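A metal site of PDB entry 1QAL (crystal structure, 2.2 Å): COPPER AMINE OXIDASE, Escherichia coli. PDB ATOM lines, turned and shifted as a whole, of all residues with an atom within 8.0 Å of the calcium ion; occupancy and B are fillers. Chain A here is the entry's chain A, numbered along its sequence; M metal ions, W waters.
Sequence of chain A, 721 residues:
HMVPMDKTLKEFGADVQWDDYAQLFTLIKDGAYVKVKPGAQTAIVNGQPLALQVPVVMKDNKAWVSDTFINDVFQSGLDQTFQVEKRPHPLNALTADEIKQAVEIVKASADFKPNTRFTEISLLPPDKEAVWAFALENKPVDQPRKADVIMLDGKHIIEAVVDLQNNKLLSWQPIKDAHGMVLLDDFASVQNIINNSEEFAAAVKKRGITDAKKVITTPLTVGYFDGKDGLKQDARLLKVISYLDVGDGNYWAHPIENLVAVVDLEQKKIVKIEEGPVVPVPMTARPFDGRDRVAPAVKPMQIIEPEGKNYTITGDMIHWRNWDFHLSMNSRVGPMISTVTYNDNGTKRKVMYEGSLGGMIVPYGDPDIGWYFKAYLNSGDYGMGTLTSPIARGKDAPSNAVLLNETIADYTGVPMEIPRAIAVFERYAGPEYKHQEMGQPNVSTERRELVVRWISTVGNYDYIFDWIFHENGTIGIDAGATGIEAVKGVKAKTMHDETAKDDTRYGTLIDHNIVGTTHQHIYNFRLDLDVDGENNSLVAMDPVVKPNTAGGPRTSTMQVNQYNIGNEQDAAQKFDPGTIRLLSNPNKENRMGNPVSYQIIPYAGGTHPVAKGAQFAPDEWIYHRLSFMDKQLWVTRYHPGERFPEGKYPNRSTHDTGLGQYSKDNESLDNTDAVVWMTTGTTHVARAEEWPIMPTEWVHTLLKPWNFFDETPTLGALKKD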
ATOM      1  N   LYS A 128      -9.228  15.646 -21.551  1.00  0.00           N
ATOM      2  CA  LYS A 128      -8.303  16.737 -21.766  1.00  0.00           C
ATOM      3  C   LYS A 128      -8.078  17.599 -20.521  1.00  0.00           C
ATOM      4  O   LYS A 128      -6.941  18.011 -20.194  1.00  0.00           O
ATOM      5  CB  LYS A 128      -8.884  17.585 -22.931  1.00  0.00           C
ATOM      6  CG  LYS A 128      -8.312  18.993 -23.088  1.00  0.00           C
ATOM      7  CD  LYS A 128      -8.731  19.492 -24.475  1.00  0.00           C
ATOM      8  CE  LYS A 128      -8.177  20.878 -24.753  1.00  0.00           C
ATOM      9  NZ  LYS A 128      -8.445  21.189 -26.193  1.00  0.00           N
ATOM     10  N   TRP A 132      -4.500  18.525 -18.719  1.00  0.00           N
ATOM     11  CA  TRP A 132      -3.924  19.865 -18.526  1.00  0.00           C
ATOM     12  C   TRP A 132      -3.667  20.116 -17.034  1.00  0.00           C
ATOM     13  O   TRP A 132      -2.630  20.717 -16.719  1.00  0.00           O
ATOM     14  CB  TRP A 132      -4.871  20.947 -19.082  1.00  0.00           C
ATOM     15  CG  TRP A 132      -4.655  21.425 -20.471  1.00  0.00           C
ATOM     16  CD1 TRP A 132      -5.590  21.550 -21.469  1.00  0.00           C
ATOM     17  CD2 TRP A 132      -3.421  21.870 -21.067  1.00  0.00           C
ATOM     18  NE1 TRP A 132      -5.045  22.039 -22.650  1.00  0.00           N
ATOM     19  CE2 TRP A 132      -3.699  22.227 -22.395  1.00  0.00           C
ATOM     20  CE3 TRP A 132      -2.117  21.975 -20.576  1.00  0.00           C
ATOM     21  CZ2 TRP A 132      -2.715  22.705 -23.282  1.00  0.00           C
ATOM     22  CZ3 TRP A 132      -1.122  22.444 -21.432  1.00  0.00           C
ATOM     23  CH2 TRP A 132      -1.461  22.792 -22.745  1.00  0.00           C
ATOM     24  N   VAL A 351      -0.582  26.598 -25.157  1.00  0.00           N
ATOM     25  CA  VAL A 351      -0.438  26.915 -26.563  1.00  0.00           C
ATOM     26  C   VAL A 351      -1.160  25.824 -27.346  1.00  0.00           C
ATOM     27  O   VAL A 351      -2.030  26.055 -28.193  1.00  0.00           O
ATOM     28  CB  VAL A 351       1.038  26.956 -26.981  1.00  0.00           C
ATOM     29  CG1 VAL A 351       1.163  27.195 -28.484  1.00  0.00           C
ATOM     30  CG2 VAL A 351       1.701  28.089 -26.226  1.00  0.00           C
ATOM     31  N   MET A 352      -0.804  24.568 -27.058  1.00  0.00           N
ATOM     32  CA  MET A 352      -1.424  23.457 -27.772  1.00  0.00           C
ATOM     33  C   MET A 352      -1.614  22.221 -26.915  1.00  0.00           C
ATOM     34  O   MET A 352      -0.722  21.656 -26.253  1.00  0.00           O
ATOM     35  CB  MET A 352      -0.495  23.034 -28.951  1.00  0.00           C
ATOM     36  CG  MET A 352      -1.116  22.014 -29.914  1.00  0.00           C
ATOM     37  SD  MET A 352      -0.256  21.785 -31.505  1.00  0.00           S
ATOM     38  CE  MET A 352       1.372  21.319 -30.907  1.00  0.00           C
ATOM     39  N   TYR A 353      -2.834  21.700 -26.895  1.00  0.00           N
ATOM     40  CA  TYR A 353      -3.104  20.480 -26.132  1.00  0.00           C
ATOM     41  C   TYR A 353      -2.515  19.289 -26.862  1.00  0.00           C
ATOM     42  O   TYR A 353      -1.827  18.439 -26.308  1.00  0.00           O
ATOM     43  CB  TYR A 353      -4.638  20.284 -25.920  1.00  0.00           C
ATOM     44  CG  TYR A 353      -4.816  18.970 -25.179  1.00  0.00           C
ATOM     45  CD1 TYR A 353      -4.381  18.846 -23.873  1.00  0.00           C
ATOM     46  CD2 TYR A 353      -5.407  17.852 -25.772  1.00  0.00           C
ATOM     47  CE1 TYR A 353      -4.534  17.648 -23.155  1.00  0.00           C
ATOM     48  CE2 TYR A 353      -5.569  16.654 -25.082  1.00  0.00           C
ATOM     49  CZ  TYR A 353      -5.131  16.575 -23.771  1.00  0.00           C
ATOM     50  OH  TYR A 353      -5.280  15.395 -23.100  1.00  0.00           O
ATOM     51  N   GLU A 354      -2.786  19.160 -28.167  1.00  0.00           N
ATOM     52  CA  GLU A 354      -2.238  18.050 -28.948  1.00  0.00           C
ATOM     53  C   GLU A 354      -2.059  18.433 -30.406  1.00  0.00           C
ATOM     54  O   GLU A 354      -2.902  19.125 -30.976  1.00  0.00           O
ATOM     55  CB  GLU A 354      -3.074  16.768 -29.050  1.00  0.00           C
ATOM     56  CG  GLU A 354      -3.559  16.211 -27.719  1.00  0.00           C
ATOM     57  CD  GLU A 354      -4.374  14.936 -27.949  1.00  0.00           C
ATOM     58  OE1 GLU A 354      -3.658  13.957 -28.241  1.00  0.00           O
ATOM     59  OE2 GLU A 354      -5.619  14.870 -27.864  1.00  0.00           O
ATOM     60  N   ARG A 526      -3.339  17.925 -37.589  1.00  0.00           N
ATOM     61  CA  ARG A 526      -4.419  18.157 -36.635  1.00  0.00           C
ATOM     62  C   ARG A 526      -3.793  18.884 -35.448  1.00  0.00           C
ATOM     63  O   ARG A 526      -3.022  18.205 -34.757  1.00  0.00           O
ATOM     64  CB  ARG A 526      -5.109  16.854 -36.205  1.00  0.00           C
ATOM     65  CG  ARG A 526      -6.075  17.082 -35.040  1.00  0.00           C
ATOM     66  CD  ARG A 526      -6.659  15.738 -34.579  1.00  0.00           C
ATOM     67  NE  ARG A 526      -7.757  15.946 -33.618  1.00  0.00           N
ATOM     68  CZ  ARG A 526      -7.444  16.265 -32.353  1.00  0.00           C
ATOM     69  NH1 ARG A 526      -6.161  16.397 -31.994  1.00  0.00           N
ATOM     70  NH2 ARG A 526      -8.400  16.460 -31.464  1.00  0.00           N
ATOM     71  N   LEU A 527      -4.129  20.144 -35.276  1.00  0.00           N
ATOM     72  CA  LEU A 527      -3.590  20.917 -34.190  1.00  0.00           C
ATOM     73  C   LEU A 527      -4.653  21.444 -33.231  1.00  0.00           C
ATOM     74  O   LEU A 527      -5.308  22.475 -33.447  1.00  0.00           O
ATOM     75  CB  LEU A 527      -2.788  22.140 -34.775  1.00  0.00           C
ATOM     76  CG  LEU A 527      -1.963  21.762 -36.042  1.00  0.00           C
ATOM     77  CD1 LEU A 527      -1.508  23.018 -36.784  1.00  0.00           C
ATOM     78  CD2 LEU A 527      -0.789  20.944 -35.488  1.00  0.00           C
ATOM     79  N   ASP A 528      -4.778  20.723 -32.123  1.00  0.00           N
ATOM     80  CA  ASP A 528      -5.731  21.170 -31.088  1.00  0.00           C
ATOM     81  C   ASP A 528      -5.051  22.273 -30.272  1.00  0.00           C
ATOM     82  O   ASP A 528      -4.581  22.102 -29.133  1.00  0.00           O
ATOM     83  CB  ASP A 528      -6.102  20.023 -30.163  1.00  0.00           C
ATOM     84  CG  ASP A 528      -6.969  20.432 -29.005  1.00  0.00           C
ATOM     85  OD1 ASP A 528      -7.526  21.526 -28.929  1.00  0.00           O
ATOM     86  OD2 ASP A 528      -7.154  19.690 -28.053  1.00  0.00           O
ATOM     87  N   LEU A 529      -5.019  23.478 -30.884  1.00  0.00           N
ATOM     88  CA  LEU A 529      -4.424  24.629 -30.227  1.00  0.00           C
ATOM     89  C   LEU A 529      -5.342  25.164 -29.110  1.00  0.00           C
ATOM     90  O   LEU A 529      -6.504  25.221 -29.432  1.00  0.00           O
ATOM     91  CB  LEU A 529      -4.273  25.757 -31.289  1.00  0.00           C
ATOM     92  CG  LEU A 529      -3.201  25.474 -32.363  1.00  0.00           C
ATOM     93  CD1 LEU A 529      -3.306  26.478 -33.502  1.00  0.00           C
ATOM     94  CD2 LEU A 529      -1.799  25.350 -31.750  1.00  0.00           C
ATOM     95  N   ASP A 530      -4.810  25.510 -27.941  1.00  0.00           N
ATOM     96  CA  ASP A 530      -5.625  26.049 -26.851  1.00  0.00           C
ATOM     97  C   ASP A 530      -4.805  27.327 -26.584  1.00  0.00           C
ATOM     98  O   ASP A 530      -3.860  27.270 -25.814  1.00  0.00           O
ATOM     99  CB  ASP A 530      -5.658  25.198 -25.610  1.00  0.00           C
ATOM    100  CG  ASP A 530      -6.483  23.926 -25.720  1.00  0.00           C
ATOM    101  OD1 ASP A 530      -7.318  23.678 -26.611  1.00  0.00           O
ATOM    102  OD2 ASP A 530      -6.309  23.072 -24.829  1.00  0.00           O
ATOM    103  N   VAL A 531      -5.180  28.430 -27.265  1.00  0.00           N
ATOM    104  CA  VAL A 531      -4.441  29.664 -27.113  1.00  0.00           C
ATOM    105  C   VAL A 531      -4.617  30.337 -25.779  1.00  0.00           C
ATOM    106  O   VAL A 531      -5.637  31.014 -25.645  1.00  0.00           O
ATOM    107  CB  VAL A 531      -4.792  30.568 -28.294  1.00  0.00           C
ATOM    108  CG1 VAL A 531      -4.151  31.941 -28.142  1.00  0.00           C
ATOM    109  CG2 VAL A 531      -4.370  29.900 -29.613  1.00  0.00           C
ATOM    110  N   GLY A 533      -5.570  29.228 -23.282  1.00  0.00           N
ATOM    111  CA  GLY A 533      -6.804  28.770 -22.626  1.00  0.00           C
ATOM    112  C   GLY A 533      -7.625  27.944 -23.586  1.00  0.00           C
ATOM    113  O   GLY A 533      -7.278  27.850 -24.775  1.00  0.00           O
ATOM    114  N   GLU A 534      -8.672  27.340 -23.042  1.00  0.00           N
ATOM    115  CA  GLU A 534      -9.591  26.504 -23.832  1.00  0.00           C
ATOM    116  C   GLU A 534     -10.466  27.185 -24.878  1.00  0.00           C
ATOM    117  O   GLU A 534     -10.521  26.854 -26.061  1.00  0.00           O
ATOM    118  CB  GLU A 534     -10.532  25.773 -22.859  1.00  0.00           C
ATOM    119  CG  GLU A 534     -11.412  24.714 -23.503  1.00  0.00           C
ATOM    120  CD  GLU A 534     -12.534  24.250 -22.578  1.00  0.00           C
ATOM    121  OE1 GLU A 534     -12.383  24.223 -21.340  1.00  0.00           O
ATOM    122  OE2 GLU A 534     -13.611  23.892 -23.080  1.00  0.00           O
ATOM    123  N   ASN A 535     -11.206  28.190 -24.455  1.00  0.00           N
ATOM    124  CA  ASN A 535     -12.150  28.953 -25.267  1.00  0.00           C
ATOM    125  C   ASN A 535     -11.524  29.980 -26.170  1.00  0.00           C
ATOM    126  O   ASN A 535     -11.000  30.965 -25.678  1.00  0.00           O
ATOM    127  CB  ASN A 535     -13.204  29.604 -24.328  1.00  0.00           C
ATOM    128  CG  ASN A 535     -13.791  28.531 -23.395  1.00  0.00           C
ATOM    129  OD1 ASN A 535     -14.132  27.445 -23.826  1.00  0.00           O
ATOM    130  ND2 ASN A 535     -13.963  28.700 -22.092  1.00  0.00           N
ATOM    131  N   ASN A 536     -11.582  29.748 -27.478  1.00  0.00           N
ATOM    132  CA  ASN A 536     -11.012  30.612 -28.481  1.00  0.00           C
ATOM    133  C   ASN A 536     -12.020  30.887 -29.595  1.00  0.00           C
ATOM    134  O   ASN A 536     -13.069  30.249 -29.551  1.00  0.00           O
ATOM    135  CB  ASN A 536      -9.757  29.963 -29.152  1.00  0.00           C
ATOM    136  CG  ASN A 536      -8.731  29.523 -28.097  1.00  0.00           C
ATOM    137  OD1 ASN A 536      -8.657  29.998 -26.946  1.00  0.00           O
ATOM    138  ND2 ASN A 536      -7.894  28.556 -28.534  1.00  0.00           N
ATOM    139  N   LEU A 583      -6.279  32.392 -34.374  1.00  0.00           N
ATOM    140  CA  LEU A 583      -7.069  31.615 -33.414  1.00  0.00           C
ATOM    141  C   LEU A 583      -6.743  32.530 -32.207  1.00  0.00           C
ATOM    142  O   LEU A 583      -5.603  32.537 -31.737  1.00  0.00           O
ATOM    143  CB  LEU A 583      -6.722  30.145 -33.214  1.00  0.00           C
ATOM    144  CG  LEU A 583      -7.611  29.491 -32.137  1.00  0.00           C
ATOM    145  CD1 LEU A 583      -9.031  29.364 -32.685  1.00  0.00           C
ATOM    146  CD2 LEU A 583      -7.150  28.100 -31.742  1.00  0.00           C
ATOM    147  N   THR A 636     -12.651  22.958 -36.250  1.00  0.00           N
ATOM    148  CA  THR A 636     -13.825  22.278 -35.723  1.00  0.00           C
ATOM    149  C   THR A 636     -13.834  22.338 -34.207  1.00  0.00           C
ATOM    150  O   THR A 636     -12.788  22.659 -33.634  1.00  0.00           O
ATOM    151  CB  THR A 636     -13.856  20.788 -36.123  1.00  0.00           C
ATOM    152  OG1 THR A 636     -12.657  20.106 -35.631  1.00  0.00           O
ATOM    153  CG2 THR A 636     -13.916  20.709 -37.649  1.00  0.00           C
ATOM    154  N   ARG A 637     -15.006  22.049 -33.668  1.00  0.00           N
ATOM    155  CA  ARG A 637     -15.256  22.024 -32.217  1.00  0.00           C
ATOM    156  C   ARG A 637     -14.505  20.800 -31.702  1.00  0.00           C
ATOM    157  O   ARG A 637     -14.603  19.763 -32.347  1.00  0.00           O
ATOM    158  CB  ARG A 637     -16.780  21.908 -32.063  1.00  0.00           C
ATOM    159  CG  ARG A 637     -17.179  21.745 -30.606  1.00  0.00           C
ATOM    160  CD  ARG A 637     -17.035  23.075 -29.916  1.00  0.00           C
ATOM    161  NE  ARG A 637     -18.185  23.618 -29.213  1.00  0.00           N
ATOM    162  CZ  ARG A 637     -19.273  23.929 -29.928  1.00  0.00           C
ATOM    163  NH1 ARG A 637     -19.245  23.747 -31.235  1.00  0.00           N
ATOM    164  NH2 ARG A 637     -20.124  24.391 -29.049  1.00  0.00           N
ATOM    165  N   TYR A 638     -13.748  20.843 -30.627  1.00  0.00           N
ATOM    166  CA  TYR A 638     -12.991  19.749 -30.078  1.00  0.00           C
ATOM    167  C   TYR A 638     -13.946  18.612 -29.685  1.00  0.00           C
ATOM    168  O   TYR A 638     -14.966  18.835 -29.031  1.00  0.00           O
ATOM    169  CB  TYR A 638     -12.176  20.173 -28.830  1.00  0.00           C
ATOM    170  CG  TYR A 638     -11.642  18.950 -28.097  1.00  0.00           C
ATOM    171  CD1 TYR A 638     -10.541  18.224 -28.569  1.00  0.00           C
ATOM    172  CD2 TYR A 638     -12.239  18.512 -26.920  1.00  0.00           C
ATOM    173  CE1 TYR A 638     -10.030  17.100 -27.915  1.00  0.00           C
ATOM    174  CE2 TYR A 638     -11.759  17.403 -26.262  1.00  0.00           C
ATOM    175  CZ  TYR A 638     -10.663  16.696 -26.740  1.00  0.00           C
ATOM    176  OH  TYR A 638     -10.237  15.595 -26.021  1.00  0.00           O
ATOM    177  N   THR A 672     -14.991  29.028 -27.965  1.00  0.00           N
ATOM    178  CA  THR A 672     -15.108  27.620 -27.587  1.00  0.00           C
ATOM    179  C   THR A 672     -13.824  26.875 -27.912  1.00  0.00           C
ATOM    180  O   THR A 672     -12.877  27.347 -28.562  1.00  0.00           O
ATOM    181  CB  THR A 672     -16.348  27.045 -28.316  1.00  0.00           C
ATOM    182  OG1 THR A 672     -16.619  25.741 -27.811  1.00  0.00           O
ATOM    183  CG2 THR A 672     -16.261  27.070 -29.819  1.00  0.00           C
ATOM    184  N   ASP A 673     -13.757  25.630 -27.458  1.00  0.00           N
ATOM    185  CA  ASP A 673     -12.591  24.786 -27.675  1.00  0.00           C
ATOM    186  C   ASP A 673     -12.465  24.413 -29.144  1.00  0.00           C
ATOM    187  O   ASP A 673     -13.171  23.550 -29.666  1.00  0.00           O
ATOM    188  CB  ASP A 673     -12.575  23.586 -26.716  1.00  0.00           C
ATOM    189  CG  ASP A 673     -11.250  22.835 -26.821  1.00  0.00           C
ATOM    190  OD1 ASP A 673     -10.367  23.076 -27.678  1.00  0.00           O
ATOM    191  OD2 ASP A 673     -11.058  21.930 -26.002  1.00  0.00           O
ATOM    192  N   ALA A 674     -11.587  25.066 -29.915  1.00  0.00           N
ATOM    193  CA  ALA A 674     -11.424  24.807 -31.354  1.00  0.00           C
ATOM    194  C   ALA A 674     -10.227  23.877 -31.594  1.00  0.00           C
ATOM    195  O   ALA A 674      -9.282  23.757 -30.823  1.00  0.00           O
ATOM    196  CB  ALA A 674     -11.041  26.102 -32.096  1.00  0.00           C
ATOM    197  N   VAL A 675     -10.235  23.204 -32.704  1.00  0.00           N
ATOM    198  CA  VAL A 675      -9.205  22.307 -33.191  1.00  0.00           C
ATOM    199  C   VAL A 675      -8.958  22.782 -34.644  1.00  0.00           C
ATOM    200  O   VAL A 675      -9.881  22.813 -35.442  1.00  0.00           O
ATOM    201  CB  VAL A 675      -9.639  20.819 -33.243  1.00  0.00           C
ATOM    202  CG1 VAL A 675      -8.546  20.019 -33.969  1.00  0.00           C
ATOM    203  CG2 VAL A 675      -9.799  20.206 -31.842  1.00  0.00           C
ATOM    204  N   VAL A 676      -7.740  23.128 -34.974  1.00  0.00           N
ATOM    205  CA  VAL A 676      -7.356  23.601 -36.295  1.00  0.00           C
ATOM    206  C   VAL A 676      -6.759  22.451 -37.099  1.00  0.00           C
ATOM    207  O   VAL A 676      -6.028  21.634 -36.540  1.00  0.00           O
ATOM    208  CB  VAL A 676      -6.264  24.680 -36.130  1.00  0.00           C
ATOM    209  CG1 VAL A 676      -5.747  25.096 -37.518  1.00  0.00           C
ATOM    210  CG2 VAL A 676      -6.838  25.832 -35.302  1.00  0.00           C
HETATM  211 CA    CA M   1      -8.349  23.720 -28.726  1.00  0.00          CA
HETATM  212  O   HOH W   1      -9.314  26.211 -28.303  1.00  0.00           O
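The side-chain carboxylate (OD2) of Asp 530 lies within salt-bridge range of the side-chain amino group (NZ) of Lys 128, 3.2 Å away.
OD2 of Asp 673 is in salt-bridge range of NZ of Lys 128.
O of Glu 354 lies within hydrogen-bond range of N of Asp 528.
The side-chain carboxylate (OD2) of Asp 528 lies within salt-bridge range of the side-chain amino group (NZ) of Lys 128, 2.7 Å away.
The indole nitrogen of Trp 132 is in hydrogen-bond range of the side-chain carboxylate of Asp 530.
The backbone carbonyl oxygen (O) of Asp 673 is in hydrogen-bond range of the backbone NH (N) of Tyr 638.
The backbone NH (N) of Asp 530 lies within hydrogen-bond range of the backbone carbonyl oxygen (O) of Val 351 (2.8 Å).
O of Asp 528 sits at hydrogen-bond distance from N of Tyr 353 (2.9 Å).
The calcium ion is bound by O of Ala 674 (2.3 Å), OD1 of Asp 528 (2.4 Å), OD1 of Asp 530 (2.4 Å), OD1 of Asp 673 (2.4 Å), O of Leu 529 (2.5 Å) and water W1 (2.7 Å).
The calcium ion has six donor atoms within binding distance.
Water W1 lies within hydrogen-bond range of the backbone carbonyl oxygen of Glu 534, the side-chain amide nitrogen of Asn 536 and the backbone NH of Ala 674.
Residues that only touch the calcium ion: Lys 128 (3.6 Å).
Of the 25 residues printed, 6 come within 4 Å of the calcium ion.
The nearest printed residue that does not touch the calcium ion is Val 675 (4.4 Å).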
